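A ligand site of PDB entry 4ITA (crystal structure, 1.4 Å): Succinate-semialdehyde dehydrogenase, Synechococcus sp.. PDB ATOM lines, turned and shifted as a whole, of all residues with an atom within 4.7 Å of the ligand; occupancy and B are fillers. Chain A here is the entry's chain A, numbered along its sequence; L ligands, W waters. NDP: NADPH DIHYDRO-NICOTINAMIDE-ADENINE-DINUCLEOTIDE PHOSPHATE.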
ATOM      1  N   VAL A 129      -5.763 -25.958 -33.042  1.00  0.00           N
ATOM      2  CA  VAL A 129      -4.719 -25.133 -32.449  1.00  0.00           C
ATOM      3  C   VAL A 129      -5.370 -24.342 -31.330  1.00  0.00           C
ATOM      4  O   VAL A 129      -6.351 -23.612 -31.547  1.00  0.00           O
ATOM      5  CB  VAL A 129      -4.108 -24.175 -33.488  1.00  0.00           C
ATOM      6  CG1 VAL A 129      -3.110 -23.225 -32.810  1.00  0.00           C
ATOM      7  CG2 VAL A 129      -3.427 -24.971 -34.591  1.00  0.00           C
ATOM      8  N   MET A 130      -4.843 -24.496 -30.115  1.00  0.00           N
ATOM      9  CA  MET A 130      -5.511 -23.993 -28.910  1.00  0.00           C
ATOM     10  C   MET A 130      -4.599 -23.103 -28.060  1.00  0.00           C
ATOM     11  O   MET A 130      -3.387 -23.204 -28.132  1.00  0.00           O
ATOM     12  CB  MET A 130      -6.032 -25.166 -28.076  1.00  0.00           C
ATOM     13  CG  MET A 130      -7.186 -25.913 -28.747  1.00  0.00           C
ATOM     14  SD  MET A 130      -8.771 -25.006 -28.833  1.00  0.00           S
ATOM     15  CE  MET A 130      -9.253 -25.325 -30.531  1.00  0.00           C
ATOM     16  N   PRO A 131      -5.203 -22.214 -27.248  1.00  0.00           N
ATOM     17  CA  PRO A 131      -4.437 -21.263 -26.440  1.00  0.00           C
ATOM     18  C   PRO A 131      -4.288 -21.684 -24.976  1.00  0.00           C
ATOM     19  O   PRO A 131      -5.011 -22.564 -24.493  1.00  0.00           O
ATOM     20  CB  PRO A 131      -5.288 -19.997 -26.530  1.00  0.00           C
ATOM     21  CG  PRO A 131      -6.665 -20.541 -26.472  1.00  0.00           C
ATOM     22  CD  PRO A 131      -6.632 -21.841 -27.277  1.00  0.00           C
ATOM     23  N   TRP A 132      -3.387 -21.020 -24.249  1.00  0.00           N
ATOM     24  CA  TRP A 132      -3.133 -21.385 -22.873  1.00  0.00           C
ATOM     25  C   TRP A 132      -4.197 -20.896 -21.887  1.00  0.00           C
ATOM     26  O   TRP A 132      -4.181 -21.321 -20.739  1.00  0.00           O
ATOM     27  CB  TRP A 132      -1.734 -20.921 -22.408  1.00  0.00           C
ATOM     28  CG  TRP A 132      -1.451 -19.481 -22.717  1.00  0.00           C
ATOM     29  CD1 TRP A 132      -0.629 -19.002 -23.710  1.00  0.00           C
ATOM     30  CD2 TRP A 132      -1.978 -18.318 -22.053  1.00  0.00           C
ATOM     31  NE1 TRP A 132      -0.609 -17.638 -23.701  1.00  0.00           N
ATOM     32  CE2 TRP A 132      -1.433 -17.188 -22.703  1.00  0.00           C
ATOM     33  CE3 TRP A 132      -2.840 -18.131 -20.973  1.00  0.00           C
ATOM     34  CZ2 TRP A 132      -1.732 -15.881 -22.296  1.00  0.00           C
ATOM     35  CZ3 TRP A 132      -3.147 -16.821 -20.587  1.00  0.00           C
ATOM     36  CH2 TRP A 132      -2.594 -15.725 -21.248  1.00  0.00           C
ATOM     37  N   ASN A 133      -5.107 -20.016 -22.294  1.00  0.00           N
ATOM     38  CA  ASN A 133      -5.942 -19.354 -21.281  1.00  0.00           C
ATOM     39  C   ASN A 133      -7.007 -20.224 -20.624  1.00  0.00           C
ATOM     40  O   ASN A 133      -7.316 -20.056 -19.449  1.00  0.00           O
ATOM     41  CB  ASN A 133      -6.489 -17.998 -21.747  1.00  0.00           C
ATOM     42  CG  ASN A 133      -7.550 -18.111 -22.807  1.00  0.00           C
ATOM     43  OD1 ASN A 133      -7.561 -19.049 -23.611  1.00  0.00           O
ATOM     44  ND2 ASN A 133      -8.467 -17.154 -22.816  1.00  0.00           N
ATOM     45  N   PHE A 134      -7.557 -21.171 -21.386  1.00  0.00           N
ATOM     46  CA  PHE A 134      -8.469 -22.169 -20.828  1.00  0.00           C
ATOM     47  C   PHE A 134      -7.977 -23.496 -21.371  1.00  0.00           C
ATOM     48  O   PHE A 134      -8.546 -24.050 -22.312  1.00  0.00           O
ATOM     49  CB  PHE A 134      -9.919 -21.908 -21.214  1.00  0.00           C
ATOM     50  CG  PHE A 134     -10.495 -20.656 -20.603  1.00  0.00           C
ATOM     51  CD1 PHE A 134     -10.511 -19.469 -21.306  1.00  0.00           C
ATOM     52  CD2 PHE A 134     -11.024 -20.677 -19.320  1.00  0.00           C
ATOM     53  CE1 PHE A 134     -11.038 -18.308 -20.739  1.00  0.00           C
ATOM     54  CE2 PHE A 134     -11.556 -19.529 -18.747  1.00  0.00           C
ATOM     55  CZ  PHE A 134     -11.557 -18.338 -19.466  1.00  0.00           C
ATOM     56  N   GLN A 138     -11.121 -25.255 -23.565  1.00  0.00           N
ATOM     57  CA  GLN A 138     -11.168 -25.007 -25.002  1.00  0.00           C
ATOM     58  C   GLN A 138     -10.889 -26.285 -25.784  1.00  0.00           C
ATOM     59  O   GLN A 138     -11.413 -26.481 -26.886  1.00  0.00           O
ATOM     60  CB  GLN A 138     -10.193 -23.926 -25.430  1.00  0.00           C
ATOM     61  CG  GLN A 138     -10.235 -22.647 -24.605  1.00  0.00           C
ATOM     62  CD  GLN A 138     -11.322 -21.723 -25.063  1.00  0.00           C
ATOM     63  OE1 GLN A 138     -12.042 -22.028 -26.004  1.00  0.00           O
ATOM     64  NE2 GLN A 138     -11.440 -20.567 -24.415  1.00  0.00           N
ATOM     65  N   ARG A 141     -14.085 -28.370 -25.545  1.00  0.00           N
ATOM     66  CA  ARG A 141     -15.087 -27.680 -26.363  1.00  0.00           C
ATOM     67  C   ARG A 141     -15.079 -28.174 -27.819  1.00  0.00           C
ATOM     68  O   ARG A 141     -16.147 -28.392 -28.405  1.00  0.00           O
ATOM     69  CB  ARG A 141     -14.877 -26.164 -26.301  1.00  0.00           C
ATOM     70  CG  ARG A 141     -15.875 -25.363 -27.126  1.00  0.00           C
ATOM     71  CD  ARG A 141     -15.696 -23.868 -26.919  1.00  0.00           C
ATOM     72  NE  ARG A 141     -14.505 -23.349 -27.589  1.00  0.00           N
ATOM     73  CZ  ARG A 141     -14.235 -22.062 -27.731  1.00  0.00           C
ATOM     74  NH1 ARG A 141     -15.048 -21.141 -27.229  1.00  0.00           N
ATOM     75  NH2 ARG A 141     -13.131 -21.669 -28.357  1.00  0.00           N
ATOM     76  N   LYS A 156      -2.538 -29.167 -31.473  1.00  0.00           N
ATOM     77  CA  LYS A 156      -1.351 -28.355 -31.213  1.00  0.00           C
ATOM     78  C   LYS A 156      -1.755 -27.340 -30.155  1.00  0.00           C
ATOM     79  O   LYS A 156      -2.473 -26.367 -30.434  1.00  0.00           O
ATOM     80  CB  LYS A 156      -0.841 -27.667 -32.480  1.00  0.00           C
ATOM     81  CG  LYS A 156       0.427 -26.823 -32.273  1.00  0.00           C
ATOM     82  CD  LYS A 156       0.137 -25.326 -32.098  1.00  0.00           C
ATOM     83  CE  LYS A 156       1.428 -24.517 -31.894  1.00  0.00           C
ATOM     84  NZ  LYS A 156       2.068 -24.748 -30.559  1.00  0.00           N
ATOM     85  N   HIS A 157      -1.352 -27.598 -28.918  1.00  0.00           N
ATOM     86  CA  HIS A 157      -1.672 -26.713 -27.811  1.00  0.00           C
ATOM     87  C   HIS A 157      -0.588 -25.641 -27.718  1.00  0.00           C
ATOM     88  O   HIS A 157       0.447 -25.715 -28.389  1.00  0.00           O
ATOM     89  CB  HIS A 157      -1.776 -27.506 -26.504  1.00  0.00           C
ATOM     90  CG  HIS A 157      -2.851 -27.015 -25.580  1.00  0.00           C
ATOM     91  ND1 HIS A 157      -3.228 -25.689 -25.532  1.00  0.00           N
ATOM     92  CD2 HIS A 157      -3.628 -27.668 -24.688  1.00  0.00           C
ATOM     93  CE1 HIS A 157      -4.195 -25.550 -24.638  1.00  0.00           C
ATOM     94  NE2 HIS A 157      -4.453 -26.734 -24.112  1.00  0.00           N
ATOM     95  N   ALA A 158      -0.834 -24.657 -26.871  1.00  0.00           N
ATOM     96  CA  ALA A 158       0.137 -23.598 -26.639  1.00  0.00           C
ATOM     97  C   ALA A 158       1.414 -24.197 -26.059  1.00  0.00           C
ATOM     98  O   ALA A 158       1.375 -25.173 -25.310  1.00  0.00           O
ATOM     99  CB  ALA A 158      -0.447 -22.567 -25.697  1.00  0.00           C
ATOM    100  N   SER A 159       2.564 -23.597 -26.389  1.00  0.00           N
ATOM    101  CA  SER A 159       3.848 -24.153 -26.000  1.00  0.00           C
ATOM    102  C   SER A 159       4.146 -24.101 -24.512  1.00  0.00           C
ATOM    103  O   SER A 159       5.065 -24.768 -24.031  1.00  0.00           O
ATOM    104  CB  SER A 159       4.978 -23.478 -26.787  1.00  0.00           C
ATOM    105  OG  SER A 159       4.984 -23.909 -28.124  1.00  0.00           O
ATOM    106  N   ILE A 187       4.432 -29.550 -30.524  1.00  0.00           N
ATOM    107  CA  ILE A 187       5.063 -28.860 -31.635  1.00  0.00           C
ATOM    108  C   ILE A 187       4.879 -27.363 -31.508  1.00  0.00           C
ATOM    109  O   ILE A 187       3.938 -26.896 -30.857  1.00  0.00           O
ATOM    110  CB  ILE A 187       4.517 -29.334 -33.002  1.00  0.00           C
ATOM    111  CG1 ILE A 187       3.027 -28.989 -33.170  1.00  0.00           C
ATOM    112  CG2 ILE A 187       4.791 -30.826 -33.218  1.00  0.00           C
ATOM    113  CD1 ILE A 187       2.452 -29.355 -34.546  1.00  0.00           C
ATOM    114  N   GLY A 188       5.788 -26.617 -32.127  1.00  0.00           N
ATOM    115  CA  GLY A 188       5.722 -25.166 -32.119  1.00  0.00           C
ATOM    116  C   GLY A 188       4.890 -24.618 -33.252  1.00  0.00           C
ATOM    117  O   GLY A 188       4.444 -25.353 -34.146  1.00  0.00           O
ATOM    118  N   ALA A 189       4.686 -23.302 -33.229  1.00  0.00           N
ATOM    119  CA  ALA A 189       3.862 -22.639 -34.230  1.00  0.00           C
ATOM    120  C   ALA A 189       4.369 -22.867 -35.659  1.00  0.00           C
ATOM    121  O   ALA A 189       3.569 -23.025 -36.590  1.00  0.00           O
ATOM    122  CB  ALA A 189       3.741 -21.149 -33.930  1.00  0.00           C
ATOM    123  N   VAL A 192       3.066 -26.102 -37.624  1.00  0.00           N
ATOM    124  CA  VAL A 192       1.652 -26.279 -37.949  1.00  0.00           C
ATOM    125  C   VAL A 192       1.410 -26.358 -39.462  1.00  0.00           C
ATOM    126  O   VAL A 192       0.534 -27.090 -39.932  1.00  0.00           O
ATOM    127  CB  VAL A 192       0.824 -25.159 -37.297  1.00  0.00           C
ATOM    128  CG1 VAL A 192      -0.625 -25.202 -37.781  1.00  0.00           C
ATOM    129  CG2 VAL A 192       0.875 -25.288 -35.796  1.00  0.00           C
ATOM    130  N   LEU A 206      -9.000 -23.050 -34.936  1.00  0.00           N
ATOM    131  CA  LEU A 206      -8.056 -22.346 -34.081  1.00  0.00           C
ATOM    132  C   LEU A 206      -8.795 -21.413 -33.133  1.00  0.00           C
ATOM    133  O   LEU A 206      -9.696 -20.666 -33.549  1.00  0.00           O
ATOM    134  CB  LEU A 206      -7.038 -21.550 -34.907  1.00  0.00           C
ATOM    135  CG  LEU A 206      -5.947 -20.804 -34.134  1.00  0.00           C
ATOM    136  CD1 LEU A 206      -4.638 -20.775 -34.906  1.00  0.00           C
ATOM    137  CD2 LEU A 206      -6.361 -19.343 -33.809  1.00  0.00           C
ATOM    138  N   THR A 207      -8.387 -21.462 -31.873  1.00  0.00           N
ATOM    139  CA  THR A 207      -8.774 -20.466 -30.878  1.00  0.00           C
ATOM    140  C   THR A 207      -7.485 -19.761 -30.463  1.00  0.00           C
ATOM    141  O   THR A 207      -6.496 -20.409 -30.114  1.00  0.00           O
ATOM    142  CB  THR A 207      -9.452 -21.139 -29.664  1.00  0.00           C
ATOM    143  OG1 THR A 207     -10.629 -21.817 -30.115  1.00  0.00           O
ATOM    144  CG2 THR A 207      -9.818 -20.109 -28.610  1.00  0.00           C
ATOM    145  N   GLY A 208      -7.474 -18.435 -30.547  1.00  0.00           N
ATOM    146  CA  GLY A 208      -6.248 -17.700 -30.345  1.00  0.00           C
ATOM    147  C   GLY A 208      -6.316 -16.266 -30.831  1.00  0.00           C
ATOM    148  O   GLY A 208      -7.403 -15.707 -30.973  1.00  0.00           O
ATOM    149  N   SER A 209      -5.154 -15.685 -31.081  1.00  0.00           N
ATOM    150  CA  SER A 209      -5.055 -14.302 -31.522  1.00  0.00           C
ATOM    151  C   SER A 209      -5.204 -14.196 -33.037  1.00  0.00           C
ATOM    152  O   SER A 209      -5.095 -15.188 -33.773  1.00  0.00           O
ATOM    153  CB  SER A 209      -3.703 -13.728 -31.118  1.00  0.00           C
ATOM    154  OG  SER A 209      -2.689 -14.265 -31.945  1.00  0.00           O
ATOM    155  N   PRO A 211      -3.149 -12.897 -35.425  1.00  0.00           N
ATOM    156  CA  PRO A 211      -2.076 -13.348 -36.319  1.00  0.00           C
ATOM    157  C   PRO A 211      -2.022 -14.871 -36.461  1.00  0.00           C
ATOM    158  O   PRO A 211      -1.761 -15.377 -37.559  1.00  0.00           O
ATOM    159  CB  PRO A 211      -0.805 -12.820 -35.651  1.00  0.00           C
ATOM    160  CG  PRO A 211      -1.262 -11.663 -34.827  1.00  0.00           C
ATOM    161  CD  PRO A 211      -2.623 -12.053 -34.327  1.00  0.00           C
ATOM    162  N   ALA A 212      -2.283 -15.600 -35.379  1.00  0.00           N
ATOM    163  CA  ALA A 212      -2.326 -17.056 -35.447  1.00  0.00           C
ATOM    164  C   ALA A 212      -3.470 -17.526 -36.360  1.00  0.00           C
ATOM    165  O   ALA A 212      -3.274 -18.379 -37.221  1.00  0.00           O
ATOM    166  CB  ALA A 212      -2.492 -17.643 -34.057  1.00  0.00           C
ATOM    167  N   SER A 215      -2.763 -16.843 -40.063  1.00  0.00           N
ATOM    168  CA  SER A 215      -1.796 -17.800 -40.577  1.00  0.00           C
ATOM    169  C   SER A 215      -2.471 -19.136 -40.899  1.00  0.00           C
ATOM    170  O   SER A 215      -2.365 -19.655 -42.010  1.00  0.00           O
ATOM    171  CB  SER A 215      -0.667 -17.986 -39.578  1.00  0.00           C
ATOM    172  OG  SER A 215       0.308 -18.875 -40.096  1.00  0.00           O
ATOM    173  N   GLU A 230     -11.957 -18.828 -33.581  1.00  0.00           N
ATOM    174  CA  GLU A 230     -12.452 -18.222 -32.356  1.00  0.00           C
ATOM    175  C   GLU A 230     -11.346 -17.302 -31.844  1.00  0.00           C
ATOM    176  O   GLU A 230     -10.384 -17.760 -31.231  1.00  0.00           O
ATOM    177  CB  GLU A 230     -12.765 -19.312 -31.328  1.00  0.00           C
ATOM    178  CG  GLU A 230     -13.919 -20.254 -31.712  1.00  0.00           C
ATOM    179  CD  GLU A 230     -15.298 -19.735 -31.304  1.00  0.00           C
ATOM    180  OE1 GLU A 230     -15.382 -18.652 -30.693  1.00  0.00           O
ATOM    181  OE2 GLU A 230     -16.299 -20.425 -31.618  1.00  0.00           O
ATOM    182  N   LEU A 231     -11.466 -16.014 -32.113  1.00  0.00           N
ATOM    183  CA  LEU A 231     -10.387 -15.087 -31.793  1.00  0.00           C
ATOM    184  C   LEU A 231     -10.756 -14.165 -30.634  1.00  0.00           C
ATOM    185  O   LEU A 231     -11.735 -14.415 -29.926  1.00  0.00           O
ATOM    186  CB  LEU A 231      -9.933 -14.306 -33.037  1.00  0.00           C
ATOM    187  CG  LEU A 231      -9.693 -15.192 -34.277  1.00  0.00           C
ATOM    188  CD1 LEU A 231      -9.290 -14.325 -35.452  1.00  0.00           C
ATOM    189  CD2 LEU A 231      -8.635 -16.303 -34.017  1.00  0.00           C
ATOM    190  N   GLY A 232      -9.973 -13.119 -30.440  1.00  0.00           N
ATOM    191  CA  GLY A 232     -10.154 -12.261 -29.281  1.00  0.00           C
ATOM    192  C   GLY A 232     -11.297 -11.270 -29.390  1.00  0.00           C
ATOM    193  O   GLY A 232     -11.970 -11.173 -30.410  1.00  0.00           O
ATOM    194  N   GLY A 233     -11.502 -10.520 -28.306  1.00  0.00           N
ATOM    195  CA  GLY A 233     -12.535  -9.510 -28.306  1.00  0.00           C
ATOM    196  C   GLY A 233     -12.168  -8.316 -27.448  1.00  0.00           C
ATOM    197  O   GLY A 233     -11.193  -8.341 -26.699  1.00  0.00           O
ATOM    198  N   SER A 263      -9.401 -13.499 -20.697  1.00  0.00           N
ATOM    199  CA  SER A 263     -10.514 -14.158 -21.355  1.00  0.00           C
ATOM    200  C   SER A 263     -10.953 -13.372 -22.566  1.00  0.00           C
ATOM    201  O   SER A 263     -11.035 -12.148 -22.538  1.00  0.00           O
ATOM    202  CB  SER A 263     -11.696 -14.326 -20.421  1.00  0.00           C
ATOM    203  OG  SER A 263     -12.791 -14.884 -21.152  1.00  0.00           O
ATOM    204  N   CYS A 264     -11.263 -14.092 -23.628  1.00  0.00           N
ATOM    205  CA  CYS A 264     -11.780 -13.493 -24.830  1.00  0.00           C
ATOM    206  C   CYS A 264     -13.096 -12.741 -24.619  1.00  0.00           C
ATOM    207  O   CYS A 264     -13.381 -11.795 -25.336  1.00  0.00           O
ATOM    208  CB  CYS A 264     -11.948 -14.580 -25.903  1.00  0.00           C
ATOM    209  SG  CYS A 264     -12.977 -15.981 -25.370  1.00  0.00           S
ATOM    210  N   ILE A 311       3.022 -11.465 -22.035  1.00  0.00           N
ATOM    211  CA  ILE A 311       1.747 -10.822 -21.750  1.00  0.00           C
ATOM    212  C   ILE A 311       1.941  -9.663 -20.785  1.00  0.00           C
ATOM    213  O   ILE A 311       1.373  -8.580 -20.974  1.00  0.00           O
ATOM    214  CB  ILE A 311       0.721 -11.818 -21.166  1.00  0.00           C
ATOM    215  CG1 ILE A 311       0.376 -12.890 -22.192  1.00  0.00           C
ATOM    216  CG2 ILE A 311      -0.534 -11.088 -20.710  1.00  0.00           C
ATOM    217  CD1 ILE A 311      -0.356 -12.351 -23.399  1.00  0.00           C
ATOM    218  N   GLU A 361      -7.050  -5.347 -27.766  1.00  0.00           N
ATOM    219  CA  GLU A 361      -7.511  -6.236 -26.711  1.00  0.00           C
ATOM    220  C   GLU A 361      -6.589  -6.123 -25.509  1.00  0.00           C
ATOM    221  O   GLU A 361      -5.371  -6.235 -25.633  1.00  0.00           O
ATOM    222  CB  GLU A 361      -7.546  -7.681 -27.186  1.00  0.00           C
ATOM    223  CG  GLU A 361      -7.988  -8.654 -26.095  1.00  0.00           C
ATOM    224  CD  GLU A 361      -8.164 -10.083 -26.576  1.00  0.00           C
ATOM    225  OE1 GLU A 361      -7.332 -10.546 -27.376  1.00  0.00           O
ATOM    226  OE2 GLU A 361      -9.136 -10.735 -26.138  1.00  0.00           O
ATOM    227  N   PHE A 363      -5.587  -8.025 -22.487  1.00  0.00           N
ATOM    228  CA  PHE A 363      -5.665  -9.411 -22.050  1.00  0.00           C
ATOM    229  C   PHE A 363      -5.020  -9.505 -20.666  1.00  0.00           C
ATOM    230  O   PHE A 363      -3.987 -10.133 -20.487  1.00  0.00           O
ATOM    231  CB  PHE A 363      -4.942 -10.300 -23.063  1.00  0.00           C
ATOM    232  CG  PHE A 363      -5.533 -11.683 -23.193  1.00  0.00           C
ATOM    233  CD1 PHE A 363      -6.861 -11.860 -23.527  1.00  0.00           C
ATOM    234  CD2 PHE A 363      -4.740 -12.803 -22.999  1.00  0.00           C
ATOM    235  CE1 PHE A 363      -7.390 -13.127 -23.657  1.00  0.00           C
ATOM    236  CE2 PHE A 363      -5.265 -14.079 -23.127  1.00  0.00           C
ATOM    237  CZ  PHE A 363      -6.590 -14.231 -23.460  1.00  0.00           C
ATOM    238  N   LEU A 389     -17.013 -10.139 -30.484  1.00  0.00           N
ATOM    239  CA  LEU A 389     -17.216 -11.435 -29.876  1.00  0.00           C
ATOM    240  C   LEU A 389     -18.459 -11.439 -28.987  1.00  0.00           C
ATOM    241  O   LEU A 389     -19.513 -11.922 -29.407  1.00  0.00           O
ATOM    242  CB  LEU A 389     -15.963 -11.861 -29.103  1.00  0.00           C
ATOM    243  CG  LEU A 389     -15.983 -13.304 -28.593  1.00  0.00           C
ATOM    244  CD1 LEU A 389     -16.352 -14.315 -29.690  1.00  0.00           C
ATOM    245  CD2 LEU A 389     -14.646 -13.624 -27.986  1.00  0.00           C
ATOM    246  N   PHE A 427     -21.549 -20.594 -29.715  1.00  0.00           N
ATOM    247  CA  PHE A 427     -20.602 -19.587 -29.252  1.00  0.00           C
ATOM    248  C   PHE A 427     -19.591 -19.277 -30.348  1.00  0.00           C
ATOM    249  O   PHE A 427     -18.900 -20.177 -30.829  1.00  0.00           O
ATOM    250  CB  PHE A 427     -19.869 -20.094 -28.013  1.00  0.00           C
ATOM    251  CG  PHE A 427     -18.919 -19.104 -27.403  1.00  0.00           C
ATOM    252  CD1 PHE A 427     -19.319 -18.300 -26.347  1.00  0.00           C
ATOM    253  CD2 PHE A 427     -17.620 -18.971 -27.884  1.00  0.00           C
ATOM    254  CE1 PHE A 427     -18.438 -17.384 -25.781  1.00  0.00           C
ATOM    255  CE2 PHE A 427     -16.741 -18.058 -27.327  1.00  0.00           C
ATOM    256  CZ  PHE A 427     -17.152 -17.260 -26.277  1.00  0.00           C
HETATM  257  PA  NDP L   1      -1.662 -16.932 -29.677  1.00  0.00           P
HETATM  258  O1A NDP L   1      -2.453 -16.700 -30.935  1.00  0.00           O
HETATM  259  O2A NDP L   1      -0.291 -16.329 -29.538  1.00  0.00           O
HETATM  260  O5B NDP L   1      -1.520 -18.505 -29.463  1.00  0.00           O
HETATM  261  C5B NDP L   1      -2.641 -19.402 -29.556  1.00  0.00           C
HETATM  262  C4B NDP L   1      -2.223 -20.720 -30.204  1.00  0.00           C
HETATM  263  O4B NDP L   1      -1.842 -20.467 -31.558  1.00  0.00           O
HETATM  264  C3B NDP L   1      -1.007 -21.360 -29.552  1.00  0.00           C
HETATM  265  O3B NDP L   1      -1.110 -22.783 -29.694  1.00  0.00           O
HETATM  266  C2B NDP L   1       0.137 -20.865 -30.409  1.00  0.00           C
HETATM  267  O2B NDP L   1       1.283 -21.698 -30.389  1.00  0.00           O
HETATM  268  C1B NDP L   1      -0.507 -20.942 -31.764  1.00  0.00           C
HETATM  269  N9A NDP L   1       0.080 -20.072 -32.799  1.00  0.00           N
HETATM  270  C8A NDP L   1       0.562 -18.823 -32.662  1.00  0.00           C
HETATM  271  N7A NDP L   1       0.978 -18.349 -33.863  1.00  0.00           N
HETATM  272  C5A NDP L   1       0.735 -19.302 -34.770  1.00  0.00           C
HETATM  273  C6A NDP L   1       0.924 -19.470 -36.222  1.00  0.00           C
HETATM  274  N6A NDP L   1       1.468 -18.485 -36.951  1.00  0.00           N
HETATM  275  N1A NDP L   1       0.540 -20.648 -36.766  1.00  0.00           N
HETATM  276  C2A NDP L   1      -0.005 -21.637 -36.047  1.00  0.00           C
HETATM  277  N3A NDP L   1      -0.211 -21.553 -34.724  1.00  0.00           N
HETATM  278  C4A NDP L   1       0.145 -20.437 -34.064  1.00  0.00           C
HETATM  279  O3  NDP L   1      -2.687 -16.455 -28.500  1.00  0.00           O
HETATM  280  PN  NDP L   1      -2.464 -15.762 -27.049  1.00  0.00           P
HETATM  281  O1N NDP L   1      -1.405 -14.691 -27.091  1.00  0.00           O
HETATM  282  O2N NDP L   1      -2.398 -16.872 -26.037  1.00  0.00           O
HETATM  283  O5D NDP L   1      -3.878 -15.015 -26.867  1.00  0.00           O
HETATM  284  C5D NDP L   1      -5.081 -15.768 -26.741  1.00  0.00           C
HETATM  285  C4D NDP L   1      -6.136 -15.224 -27.690  1.00  0.00           C
HETATM  286  O4D NDP L   1      -7.175 -16.186 -27.866  1.00  0.00           O
HETATM  287  C3D NDP L   1      -6.810 -13.970 -27.166  1.00  0.00           C
HETATM  288  O3D NDP L   1      -6.966 -13.014 -28.232  1.00  0.00           O
HETATM  289  C2D NDP L   1      -8.130 -14.522 -26.672  1.00  0.00           C
HETATM  290  O2D NDP L   1      -9.115 -13.486 -26.606  1.00  0.00           O
HETATM  291  C1D NDP L   1      -8.457 -15.550 -27.729  1.00  0.00           C
HETATM  292  N1N NDP L   1      -9.477 -16.487 -27.232  1.00  0.00           N
HETATM  293  C2N NDP L   1     -10.534 -16.804 -28.004  1.00  0.00           C
HETATM  294  C3N NDP L   1     -11.701 -17.277 -27.411  1.00  0.00           C
HETATM  295  C7N NDP L   1     -12.896 -17.666 -28.233  1.00  0.00           C
HETATM  296  O7N NDP L   1     -13.458 -18.725 -27.973  1.00  0.00           O
HETATM  297  N7N NDP L   1     -13.309 -16.877 -29.212  1.00  0.00           N
HETATM  298  C4N NDP L   1     -11.821 -17.389 -25.908  1.00  0.00           C
HETATM  299  C5N NDP L   1     -10.487 -17.493 -25.322  1.00  0.00           C
HETATM  300  C6N NDP L   1      -9.371 -17.033 -26.008  1.00  0.00           C
HETATM  301  P2B NDP L   1       2.578 -21.339 -29.504  1.00  0.00           P
HETATM  302  O1X NDP L   1       3.495 -22.487 -29.807  1.00  0.00           O
HETATM  303  O2X NDP L   1       3.097 -20.015 -30.010  1.00  0.00           O
HETATM  304  O3X NDP L   1       2.163 -21.303 -28.061  1.00  0.00           O
HETATM  305  O   HOH W   1       4.033 -19.737 -26.534  1.00  0.00           O
HETATM  306  O   HOH W   2       5.829 -21.885 -31.066  1.00  0.00           O
HETATM  307  O   HOH W   3       1.267 -16.892 -27.721  1.00  0.00           O
HETATM  308  O   HOH W   4      -1.912 -19.386 -26.318  1.00  0.00           O
HETATM  309  O   HOH W   5       0.938 -21.634 -39.355  1.00  0.00           O
HETATM  310  O   HOH W   6       0.827 -19.323 -26.826  1.00  0.00           O
HETATM  311  O   HOH W   7       0.633 -15.750 -25.525  1.00  0.00           O
HETATM  312  O   HOH W   8      -4.242 -17.525 -24.102  1.00  0.00           O
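An oxygen (O4D) of the ligand sits close to the backbone carbonyl oxygen (O) of Gly 208 (3.2 Å). Residues that only touch the ligand: Val 129 (3.3 Å), Asn 133 (3.2 Å), Gln 138 (3.3 Å), His 157 (3.5 Å), Ala 189 (3.6 Å), Val 192 (3.8 Å), Thr 207 (3.4 Å), Ala 212 (3.3 Å), Gly 232 (3.1 Å), Phe 363 (3.4 Å), Leu 389 (3.7 Å) and Phe 427 (3.4 Å). The nearest printed residue that does not touch the ligand is Pro 131 (4.05 Å).
The backbone NH (N) of Ser 209 sits at hydrogen-bond distance from an oxygen (O1A) of the ligand (2.9 Å). The side-chain hydroxyl of Ser 159 sits at hydrogen-bond distance from an oxygen (O1X) of the ligand, at 2.7 Å. N7N of the ligand is in hydrogen-bond range of OE1 of Glu 230 (3.1 Å). O3D of the ligand lies within hydrogen-bond range of OE1 of Glu 361, at 2.6 Å. NE1 of Trp 132 sits at hydrogen-bond distance from O2N of the ligand. The guanidinium group of Arg 141 sits at hydrogen-bond distance from an oxygen (O7N) of the ligand. N of Ser 159 is in hydrogen-bond range of O3X of the ligand (2.9 Å). NZ of Lys 156 lies within salt-bridge range of O1X of the ligand, at 2.8 Å. An oxygen (O3B) of the ligand is in hydrogen-bond range of the backbone carbonyl oxygen of Met 130, at 2.8 Å. An oxygen (O1A) of the ligand is in hydrogen-bond range of the side-chain hydroxyl (OG) of Ser 209 (2.6 Å). A carbon (C4N) of the ligand is bonded to the side-chain sulfur (SG) of Cys 264 (1.9 Å). N6A of the ligand is in hydrogen-bond range of OG of Ser 215 (3.4 Å). O of Leu 231 is in hydrogen-bond range of N7N of the ligand. The backbone NH (N) of Ala 158 lies close to an oxygen (O3B) of the ligand, 3.4 Å away.
Water W4 lies within hydrogen-bond range of an oxygen (O2N) of the ligand (2.6 Å) and the backbone NH of Trp 132 (3.0 Å). Water W2 lies within hydrogen-bond range of an oxygen (O1X) of the ligand and the backbone NH (N) of Ala 189. Water W8 bridges an oxygen (O2N) of the ligand and the backbone NH (N) of Asn 133. Water W7 lies within hydrogen-bond range of an oxygen (O1N) of the ligand (2.8 Å) and the indole nitrogen (NE1) of Trp 132 (2.9 Å). Water W5 bridges N1A of the ligand (2.8 Å) and OG of Ser 215 (2.9 Å).
The backbone NH (N) of Ala 158 is in hydrogen-bond range of the backbone carbonyl oxygen (O) of Met 130 (3.2 Å). The backbone NH (N) of Glu 230 lies within hydrogen-bond range of the backbone carbonyl oxygen (O) of Leu 206, 2.9 Å away. The backbone carbonyl oxygen (O) of Val 129 sits at hydrogen-bond distance from the backbone NH (N) of Thr 207. The guanidinium group of Arg 141 is in hydrogen-bond range of the side-chain hydroxyl of Thr 207 (3.1 Å). The side-chain amino group of Lys 156 sits at hydrogen-bond distance from the backbone carbonyl oxygen of Ile 187, at 2.9 Å. OE2 of Glu 361 sits at hydrogen-bond distance from N of Gly 233 (3.2 Å). O of Lys 156 sits at hydrogen-bond distance from N of Met 130, at 3.0 Å. The backbone carbonyl oxygen (O) of Glu 230 sits at hydrogen-bond distance from the backbone NH (N) of Gly 208 (3.1 Å).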
